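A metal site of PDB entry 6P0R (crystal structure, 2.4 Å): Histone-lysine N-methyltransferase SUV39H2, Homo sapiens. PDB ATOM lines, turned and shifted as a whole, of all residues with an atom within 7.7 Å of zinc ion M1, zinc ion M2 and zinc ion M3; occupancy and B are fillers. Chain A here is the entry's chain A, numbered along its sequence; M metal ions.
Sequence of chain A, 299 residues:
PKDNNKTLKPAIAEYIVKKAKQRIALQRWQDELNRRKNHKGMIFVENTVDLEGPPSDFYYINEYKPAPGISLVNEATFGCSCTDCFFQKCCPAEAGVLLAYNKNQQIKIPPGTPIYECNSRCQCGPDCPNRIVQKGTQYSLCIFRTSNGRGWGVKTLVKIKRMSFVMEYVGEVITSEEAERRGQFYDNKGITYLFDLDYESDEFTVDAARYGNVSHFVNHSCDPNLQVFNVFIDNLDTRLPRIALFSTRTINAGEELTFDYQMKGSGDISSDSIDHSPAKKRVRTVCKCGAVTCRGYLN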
ATOM      1  N   PHE A  78     -33.968  22.234 -16.019  1.00  0.00           N
ATOM      2  CA  PHE A  78     -32.892  23.109 -15.541  1.00  0.00           C
ATOM      3  C   PHE A  78     -32.621  22.935 -14.046  1.00  0.00           C
ATOM      4  O   PHE A  78     -33.541  22.731 -13.251  1.00  0.00           O
ATOM      5  CB  PHE A  78     -33.225  24.585 -15.803  1.00  0.00           C
ATOM      6  CG  PHE A  78     -33.201  24.956 -17.256  1.00  0.00           C
ATOM      7  CD1 PHE A  78     -31.991  25.021 -17.947  1.00  0.00           C
ATOM      8  CD2 PHE A  78     -34.391  25.231 -17.947  1.00  0.00           C
ATOM      9  CE1 PHE A  78     -31.956  25.353 -19.304  1.00  0.00           C
ATOM     10  CE2 PHE A  78     -34.359  25.577 -19.294  1.00  0.00           C
ATOM     11  CZ  PHE A  78     -33.152  25.642 -19.976  1.00  0.00           C
ATOM     12  N   GLY A  79     -31.346  23.009 -13.684  1.00  0.00           N
ATOM     13  CA  GLY A  79     -30.909  22.976 -12.296  1.00  0.00           C
ATOM     14  C   GLY A  79     -30.036  24.174 -12.007  1.00  0.00           C
ATOM     15  O   GLY A  79     -30.017  25.136 -12.781  1.00  0.00           O
ATOM     16  N   CYS A  80     -29.344  24.123 -10.894  1.00  0.00           N
ATOM     17  CA  CYS A  80     -28.441  25.196 -10.487  1.00  0.00           C
ATOM     18  C   CYS A  80     -27.060  24.932 -11.008  1.00  0.00           C
ATOM     19  O   CYS A  80     -26.778  23.839 -11.504  1.00  0.00           O
ATOM     20  CB  CYS A  80     -28.389  25.303  -8.980  1.00  0.00           C
ATOM     21  SG  CYS A  80     -27.775  23.826  -8.125  1.00  0.00           S
ATOM     22  N   SER A  81     -26.196  25.933 -10.904  1.00  0.00           N
ATOM     23  CA  SER A  81     -24.800  25.825 -11.271  1.00  0.00           C
ATOM     24  C   SER A  81     -23.874  26.283 -10.121  1.00  0.00           C
ATOM     25  O   SER A  81     -22.733  26.709 -10.365  1.00  0.00           O
ATOM     26  CB  SER A  81     -24.505  26.663 -12.524  1.00  0.00           C
ATOM     27  OG  SER A  81     -25.508  26.513 -13.509  1.00  0.00           O
ATOM     28  N   CYS A  82     -24.359  26.179  -8.856  1.00  0.00           N
ATOM     29  CA  CYS A  82     -23.528  26.498  -7.694  1.00  0.00           C
ATOM     30  C   CYS A  82     -22.309  25.579  -7.636  1.00  0.00           C
ATOM     31  O   CYS A  82     -22.374  24.415  -8.070  1.00  0.00           O
ATOM     32  CB  CYS A  82     -24.306  26.334  -6.353  1.00  0.00           C
ATOM     33  SG  CYS A  82     -26.054  26.698  -6.362  1.00  0.00           S
ATOM     34  N   THR A  83     -21.213  26.091  -7.091  1.00  0.00           N
ATOM     35  CA  THR A  83     -20.119  25.245  -6.608  1.00  0.00           C
ATOM     36  C   THR A  83     -20.316  24.905  -5.107  1.00  0.00           C
ATOM     37  O   THR A  83     -19.861  23.858  -4.645  1.00  0.00           O
ATOM     38  CB  THR A  83     -18.743  25.899  -6.854  1.00  0.00           C
ATOM     39  OG1 THR A  83     -18.705  27.185  -6.247  1.00  0.00           O
ATOM     40  CG2 THR A  83     -18.496  26.053  -8.347  1.00  0.00           C
ATOM     41  N   ASP A  84     -20.999  25.809  -4.372  1.00  0.00           N
ATOM     42  CA  ASP A  84     -21.422  25.585  -2.969  1.00  0.00           C
ATOM     43  C   ASP A  84     -22.933  25.866  -2.835  1.00  0.00           C
ATOM     44  O   ASP A  84     -23.353  27.011  -2.674  1.00  0.00           O
ATOM     45  CB  ASP A  84     -20.634  26.506  -2.008  1.00  0.00           C
ATOM     46  CG  ASP A  84     -20.957  26.241  -0.518  1.00  0.00           C
ATOM     47  OD1 ASP A  84     -22.111  25.834  -0.195  1.00  0.00           O
ATOM     48  OD2 ASP A  84     -20.077  26.456   0.333  1.00  0.00           O
ATOM     49  N   CYS A  85     -23.737  24.798  -2.873  1.00  0.00           N
ATOM     50  CA  CYS A  85     -25.198  24.949  -2.863  1.00  0.00           C
ATOM     51  C   CYS A  85     -25.781  25.439  -1.534  1.00  0.00           C
ATOM     52  O   CYS A  85     -26.932  25.892  -1.495  1.00  0.00           O
ATOM     53  CB  CYS A  85     -25.858  23.635  -3.253  1.00  0.00           C
ATOM     54  SG  CYS A  85     -25.717  23.242  -4.998  1.00  0.00           S
ATOM     55  N   PHE A  86     -25.010  25.330  -0.452  1.00  0.00           N
ATOM     56  CA  PHE A  86     -25.448  25.839   0.854  1.00  0.00           C
ATOM     57  C   PHE A  86     -25.399  27.372   0.902  1.00  0.00           C
ATOM     58  O   PHE A  86     -26.349  28.010   1.342  1.00  0.00           O
ATOM     59  CB  PHE A  86     -24.583  25.237   1.988  1.00  0.00           C
ATOM     60  CG  PHE A  86     -25.052  25.595   3.364  1.00  0.00           C
ATOM     61  CD1 PHE A  86     -26.161  24.966   3.931  1.00  0.00           C
ATOM     62  CD2 PHE A  86     -24.380  26.570   4.110  1.00  0.00           C
ATOM     63  CE1 PHE A  86     -26.595  25.306   5.202  1.00  0.00           C
ATOM     64  CE2 PHE A  86     -24.810  26.917   5.393  1.00  0.00           C
ATOM     65  CZ  PHE A  86     -25.928  26.274   5.936  1.00  0.00           C
ATOM     66  N   GLN A  88     -24.680  29.543  -1.885  1.00  0.00           N
ATOM     67  CA  GLN A  88     -25.131  30.229  -3.103  1.00  0.00           C
ATOM     68  C   GLN A  88     -26.657  30.160  -3.262  1.00  0.00           C
ATOM     69  O   GLN A  88     -27.299  29.245  -2.756  1.00  0.00           O
ATOM     70  CB  GLN A  88     -24.454  29.640  -4.328  1.00  0.00           C
ATOM     71  CG  GLN A  88     -22.957  29.822  -4.349  1.00  0.00           C
ATOM     72  CD  GLN A  88     -22.351  29.409  -5.670  1.00  0.00           C
ATOM     73  OE1 GLN A  88     -21.652  28.382  -5.763  1.00  0.00           O
ATOM     74  NE2 GLN A  88     -22.623  30.183  -6.723  1.00  0.00           N
ATOM     75  N   LYS A  89     -27.211  31.149  -3.970  1.00  0.00           N
ATOM     76  CA  LYS A  89     -28.624  31.135  -4.356  1.00  0.00           C
ATOM     77  C   LYS A  89     -28.808  29.972  -5.309  1.00  0.00           C
ATOM     78  O   LYS A  89     -28.235  29.947  -6.400  1.00  0.00           O
ATOM     79  CB  LYS A  89     -29.063  32.459  -5.013  1.00  0.00           C
ATOM     80  CG  LYS A  89     -29.396  33.557  -4.023  1.00  0.00           C
ATOM     81  CD  LYS A  89     -29.559  34.909  -4.689  1.00  0.00           C
ATOM     82  CE  LYS A  89     -30.822  34.972  -5.551  1.00  0.00           C
ATOM     83  NZ  LYS A  89     -31.220  36.381  -5.853  1.00  0.00           N
ATOM     84  N   CYS A  90     -29.642  29.029  -4.886  1.00  0.00           N
ATOM     85  CA  CYS A  90     -29.638  27.689  -5.411  1.00  0.00           C
ATOM     86  C   CYS A  90     -31.061  27.369  -5.912  1.00  0.00           C
ATOM     87  O   CYS A  90     -31.872  28.274  -6.101  1.00  0.00           O
ATOM     88  CB  CYS A  90     -29.186  26.752  -4.283  1.00  0.00           C
ATOM     89  SG  CYS A  90     -28.997  25.006  -4.678  1.00  0.00           S
ATOM     90  N   CYS A  91     -31.334  26.082  -6.158  1.00  0.00           N
ATOM     91  CA  CYS A  91     -32.672  25.616  -6.610  1.00  0.00           C
ATOM     92  C   CYS A  91     -33.854  26.204  -5.799  1.00  0.00           C
ATOM     93  O   CYS A  91     -34.814  26.711  -6.391  1.00  0.00           O
ATOM     94  CB  CYS A  91     -32.719  24.070  -6.668  1.00  0.00           C
ATOM     95  SG  CYS A  91     -31.778  23.332  -8.055  1.00  0.00           S
ATOM     96  N   PRO A  92     -33.777  26.195  -4.433  1.00  0.00           N
ATOM     97  CA  PRO A  92     -34.847  26.794  -3.602  1.00  0.00           C
ATOM     98  C   PRO A  92     -35.097  28.283  -3.894  1.00  0.00           C
ATOM     99  O   PRO A  92     -36.265  28.694  -4.047  1.00  0.00           O
ATOM    100  CB  PRO A  92     -34.333  26.608  -2.167  1.00  0.00           C
ATOM    101  CG  PRO A  92     -33.350  25.503  -2.239  1.00  0.00           C
ATOM    102  CD  PRO A  92     -32.711  25.606  -3.588  1.00  0.00           C
ATOM    103  N   TYR A 116     -37.354  22.050  -2.173  1.00  0.00           N
ATOM    104  CA  TYR A 116     -36.863  21.988  -3.535  1.00  0.00           C
ATOM    105  C   TYR A 116     -35.423  21.539  -3.507  1.00  0.00           C
ATOM    106  O   TYR A 116     -34.524  22.310  -3.152  1.00  0.00           O
ATOM    107  CB  TYR A 116     -37.017  23.341  -4.240  1.00  0.00           C
ATOM    108  CG  TYR A 116     -38.422  23.580  -4.761  1.00  0.00           C
ATOM    109  CD1 TYR A 116     -39.405  24.156  -3.960  1.00  0.00           C
ATOM    110  CD2 TYR A 116     -38.768  23.219  -6.075  1.00  0.00           C
ATOM    111  CE1 TYR A 116     -40.690  24.376  -4.440  1.00  0.00           C
ATOM    112  CE2 TYR A 116     -40.048  23.440  -6.574  1.00  0.00           C
ATOM    113  CZ  TYR A 116     -41.015  24.008  -5.748  1.00  0.00           C
ATOM    114  OH  TYR A 116     -42.297  24.228  -6.238  1.00  0.00           O
ATOM    115  N   GLU A 117     -35.209  20.265  -3.851  1.00  0.00           N
ATOM    116  CA  GLU A 117     -33.871  19.686  -3.864  1.00  0.00           C
ATOM    117  C   GLU A 117     -33.254  19.854  -5.207  1.00  0.00           C
ATOM    118  O   GLU A 117     -33.943  20.141  -6.189  1.00  0.00           O
ATOM    119  CB  GLU A 117     -33.905  18.201  -3.493  1.00  0.00           C
ATOM    120  CG  GLU A 117     -34.483  17.931  -2.091  1.00  0.00           C
ATOM    121  CD  GLU A 117     -33.999  16.643  -1.463  1.00  0.00           C
ATOM    122  OE1 GLU A 117     -33.393  15.790  -2.155  1.00  0.00           O
ATOM    123  OE2 GLU A 117     -34.218  16.484  -0.242  1.00  0.00           O
ATOM    124  N   CYS A 118     -31.933  19.694  -5.243  1.00  0.00           N
ATOM    125  CA  CYS A 118     -31.183  19.607  -6.485  1.00  0.00           C
ATOM    126  C   CYS A 118     -31.544  18.333  -7.199  1.00  0.00           C
ATOM    127  O   CYS A 118     -31.979  17.358  -6.567  1.00  0.00           O
ATOM    128  CB  CYS A 118     -29.686  19.650  -6.190  1.00  0.00           C
ATOM    129  SG  CYS A 118     -29.170  21.267  -5.684  1.00  0.00           S
ATOM    130  N   ASN A 119     -31.342  18.333  -8.512  1.00  0.00           N
ATOM    131  CA  ASN A 119     -31.896  17.311  -9.403  1.00  0.00           C
ATOM    132  C   ASN A 119     -30.832  16.846 -10.418  1.00  0.00           C
ATOM    133  O   ASN A 119     -29.669  17.194 -10.285  1.00  0.00           O
ATOM    134  CB  ASN A 119     -33.193  17.836 -10.074  1.00  0.00           C
ATOM    135  CG  ASN A 119     -32.991  19.146 -10.830  1.00  0.00           C
ATOM    136  OD1 ASN A 119     -32.288  19.193 -11.822  1.00  0.00           O
ATOM    137  ND2 ASN A 119     -33.637  20.221 -10.349  1.00  0.00           N
ATOM    138  N   ARG A 121     -30.343  17.736 -13.419  1.00  0.00           N
ATOM    139  CA  ARG A 121     -29.900  18.818 -14.283  1.00  0.00           C
ATOM    140  C   ARG A 121     -28.966  19.808 -13.561  1.00  0.00           C
ATOM    141  O   ARG A 121     -28.396  20.673 -14.191  1.00  0.00           O
ATOM    142  CB  ARG A 121     -31.120  19.585 -14.854  1.00  0.00           C
ATOM    143  CG  ARG A 121     -32.266  18.692 -15.371  1.00  0.00           C
ATOM    144  CD  ARG A 121     -32.207  18.440 -16.874  1.00  0.00           C
ATOM    145  NE  ARG A 121     -30.911  17.972 -17.351  1.00  0.00           N
ATOM    146  CZ  ARG A 121     -30.517  16.690 -17.409  1.00  0.00           C
ATOM    147  NH1 ARG A 121     -29.289  16.398 -17.857  1.00  0.00           N
ATOM    148  NH2 ARG A 121     -31.323  15.684 -17.011  1.00  0.00           N
ATOM    149  N   CYS A 122     -28.834  19.678 -12.225  1.00  0.00           N
ATOM    150  CA  CYS A 122     -27.889  20.510 -11.453  1.00  0.00           C
ATOM    151  C   CYS A 122     -26.470  20.015 -11.680  1.00  0.00           C
ATOM    152  O   CYS A 122     -26.271  18.846 -11.983  1.00  0.00           O
ATOM    153  CB  CYS A 122     -28.213  20.492  -9.955  1.00  0.00           C
ATOM    154  SG  CYS A 122     -29.798  21.208  -9.455  1.00  0.00           S
ATOM    155  N   GLN A 123     -25.499  20.897 -11.500  1.00  0.00           N
ATOM    156  CA  GLN A 123     -24.079  20.541 -11.661  1.00  0.00           C
ATOM    157  C   GLN A 123     -23.494  19.838 -10.450  1.00  0.00           C
ATOM    158  O   GLN A 123     -22.566  19.026 -10.579  1.00  0.00           O
ATOM    159  CB  GLN A 123     -23.230  21.791 -11.988  1.00  0.00           C
ATOM    160  CG  GLN A 123     -23.642  22.513 -13.267  1.00  0.00           C
ATOM    161  CD  GLN A 123     -23.631  21.595 -14.481  1.00  0.00           C
ATOM    162  OE1 GLN A 123     -22.713  20.806 -14.654  1.00  0.00           O
ATOM    163  NE2 GLN A 123     -24.676  21.687 -15.305  1.00  0.00           N
ATOM    164  N   CYS A 124     -24.010  20.154  -9.263  1.00  0.00           N
ATOM    165  CA  CYS A 124     -23.489  19.593  -8.013  1.00  0.00           C
ATOM    166  C   CYS A 124     -23.576  18.050  -7.947  1.00  0.00           C
ATOM    167  O   CYS A 124     -24.518  17.443  -8.505  1.00  0.00           O
ATOM    168  CB  CYS A 124     -24.215  20.212  -6.821  1.00  0.00           C
ATOM    169  SG  CYS A 124     -26.000  19.883  -6.839  1.00  0.00           S
ATOM    170  N   GLY A 125     -22.593  17.427  -7.290  1.00  0.00           N
ATOM    171  CA  GLY A 125     -22.559  15.968  -7.086  1.00  0.00           C
ATOM    172  C   GLY A 125     -23.450  15.496  -5.940  1.00  0.00           C
ATOM    173  O   GLY A 125     -24.169  16.299  -5.331  1.00  0.00           O
ATOM    174  N   ASP A 127     -22.843  14.548  -2.887  1.00  0.00           N
ATOM    175  CA  ASP A 127     -22.496  15.193  -1.596  1.00  0.00           C
ATOM    176  C   ASP A 127     -23.112  16.601  -1.345  1.00  0.00           C
ATOM    177  O   ASP A 127     -22.882  17.186  -0.284  1.00  0.00           O
ATOM    178  CB  ASP A 127     -20.953  15.231  -1.392  1.00  0.00           C
ATOM    179  CG  ASP A 127     -20.197  15.794  -2.624  1.00  0.00           C
ATOM    180  OD1 ASP A 127     -20.347  15.230  -3.736  1.00  0.00           O
ATOM    181  OD2 ASP A 127     -19.435  16.759  -2.444  1.00  0.00           O
ATOM    182  N   CYS A 128     -23.885  17.130  -2.311  1.00  0.00           N
ATOM    183  CA  CYS A 128     -24.621  18.388  -2.128  1.00  0.00           C
ATOM    184  C   CYS A 128     -25.554  18.318  -0.908  1.00  0.00           C
ATOM    185  O   CYS A 128     -26.294  17.356  -0.781  1.00  0.00           O
ATOM    186  CB  CYS A 128     -25.445  18.724  -3.393  1.00  0.00           C
ATOM    187  SG  CYS A 128     -26.598  20.127  -3.192  1.00  0.00           S
ATOM    188  N   PRO A 129     -25.512  19.339  -0.018  1.00  0.00           N
ATOM    189  CA  PRO A 129     -26.364  19.324   1.184  1.00  0.00           C
ATOM    190  C   PRO A 129     -27.859  19.563   0.918  1.00  0.00           C
ATOM    191  O   PRO A 129     -28.656  19.388   1.829  1.00  0.00           O
ATOM    192  CB  PRO A 129     -25.777  20.453   2.046  1.00  0.00           C
ATOM    193  CG  PRO A 129     -25.179  21.393   1.073  1.00  0.00           C
ATOM    194  CD  PRO A 129     -24.648  20.543  -0.053  1.00  0.00           C
ATOM    195  N   ASN A 130     -28.224  19.971  -0.306  1.00  0.00           N
ATOM    196  CA  ASN A 130     -29.613  19.974  -0.778  1.00  0.00           C
ATOM    197  C   ASN A 130     -30.007  18.682  -1.563  1.00  0.00           C
ATOM    198  O   ASN A 130     -30.957  18.693  -2.343  1.00  0.00           O
ATOM    199  CB  ASN A 130     -29.861  21.230  -1.666  1.00  0.00           C
ATOM    200  CG  ASN A 130     -31.336  21.605  -1.767  1.00  0.00           C
ATOM    201  OD1 ASN A 130     -32.116  21.379  -0.843  1.00  0.00           O
ATOM    202  ND2 ASN A 130     -31.716  22.208  -2.906  1.00  0.00           N
ATOM    203  N   ARG A 131     -29.257  17.587  -1.365  1.00  0.00           N
ATOM    204  CA  ARG A 131     -29.615  16.257  -1.903  1.00  0.00           C
ATOM    205  C   ARG A 131     -29.781  15.256  -0.745  1.00  0.00           C
ATOM    206  O   ARG A 131     -28.848  14.520  -0.416  1.00  0.00           O
ATOM    207  CB  ARG A 131     -28.543  15.763  -2.896  1.00  0.00           C
ATOM    208  CG  ARG A 131     -28.480  16.497  -4.224  1.00  0.00           C
ATOM    209  CD  ARG A 131     -27.454  15.845  -5.120  1.00  0.00           C
ATOM    210  NE  ARG A 131     -27.178  16.570  -6.370  1.00  0.00           N
ATOM    211  CZ  ARG A 131     -27.907  16.488  -7.498  1.00  0.00           C
ATOM    212  NH1 ARG A 131     -29.034  15.768  -7.539  1.00  0.00           N
ATOM    213  NH2 ARG A 131     -27.515  17.162  -8.585  1.00  0.00           N
HETATM  214 ZN    ZN M   1     -29.638  22.587  -7.581  1.00  0.00          ZN
HETATM  215 ZN    ZN M   2     -27.169  24.699  -6.096  1.00  0.00          ZN
HETATM  216 ZN    ZN M   3     -26.889  21.263  -5.233  1.00  0.00          ZN
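Zinc ion M2 is bound by SG of Cys 80 (2.3 Å), SG of Cys 82 (2.3 Å), SG of Cys 85 (2.3 Å) and SG of Cys 90 (2.3 Å).
SG of Cys 80 binds zinc ion M1 (2.3 Å).
The side-chain sulfur (SG) of Cys 91 binds zinc ion M1 (2.3 Å).
Zinc ion M1 is bound by SG of Cys 122.
Zinc ion M1 is bound by SG of Cys 118, 2.4 Å away.
Zinc ion M1 has four donor atoms within binding distance.
Zinc ion M3 is bound by SG of Cys 124 (2.3 Å), SG of Cys 85 (2.3 Å), SG of Cys 118 (2.3 Å) and SG of Cys 128 (2.4 Å).
The backbone carbonyl oxygen of Cys 80 lies within hydrogen-bond range of the backbone NH of Gln 123, 3.2 Å away.
The guanidinium group of Arg 131 lies within hydrogen-bond range of the backbone carbonyl oxygen of Cys 124, at 3.0 Å.
The backbone NH of Cys 118 sits at hydrogen-bond distance from the backbone carbonyl oxygen of Asn 130.
The backbone carbonyl oxygen (O) of Cys 118 lies within hydrogen-bond range of the guanidinium group (NH1) of Arg 131, 3.5 Å away.
The side-chain sulfur (SG) of Cys 122 sits close to the backbone NH (N) of Asn 119 (3.4 Å).
The side-chain sulfur (SG) of Cys 128 lies close to the backbone NH (N) of Asn 130.
Five residues have an atom within 4 Å of zinc ion M1: Cys 80, Cys 90, Cys 91, Cys 118 and Cys 122.
Of the 28 residues printed, 5 come within 4 Å of zinc ion M2.
Within 4 Å of zinc ion M3: Cys 80, Cys 85, Cys 118, Cys 124 and Cys 128.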
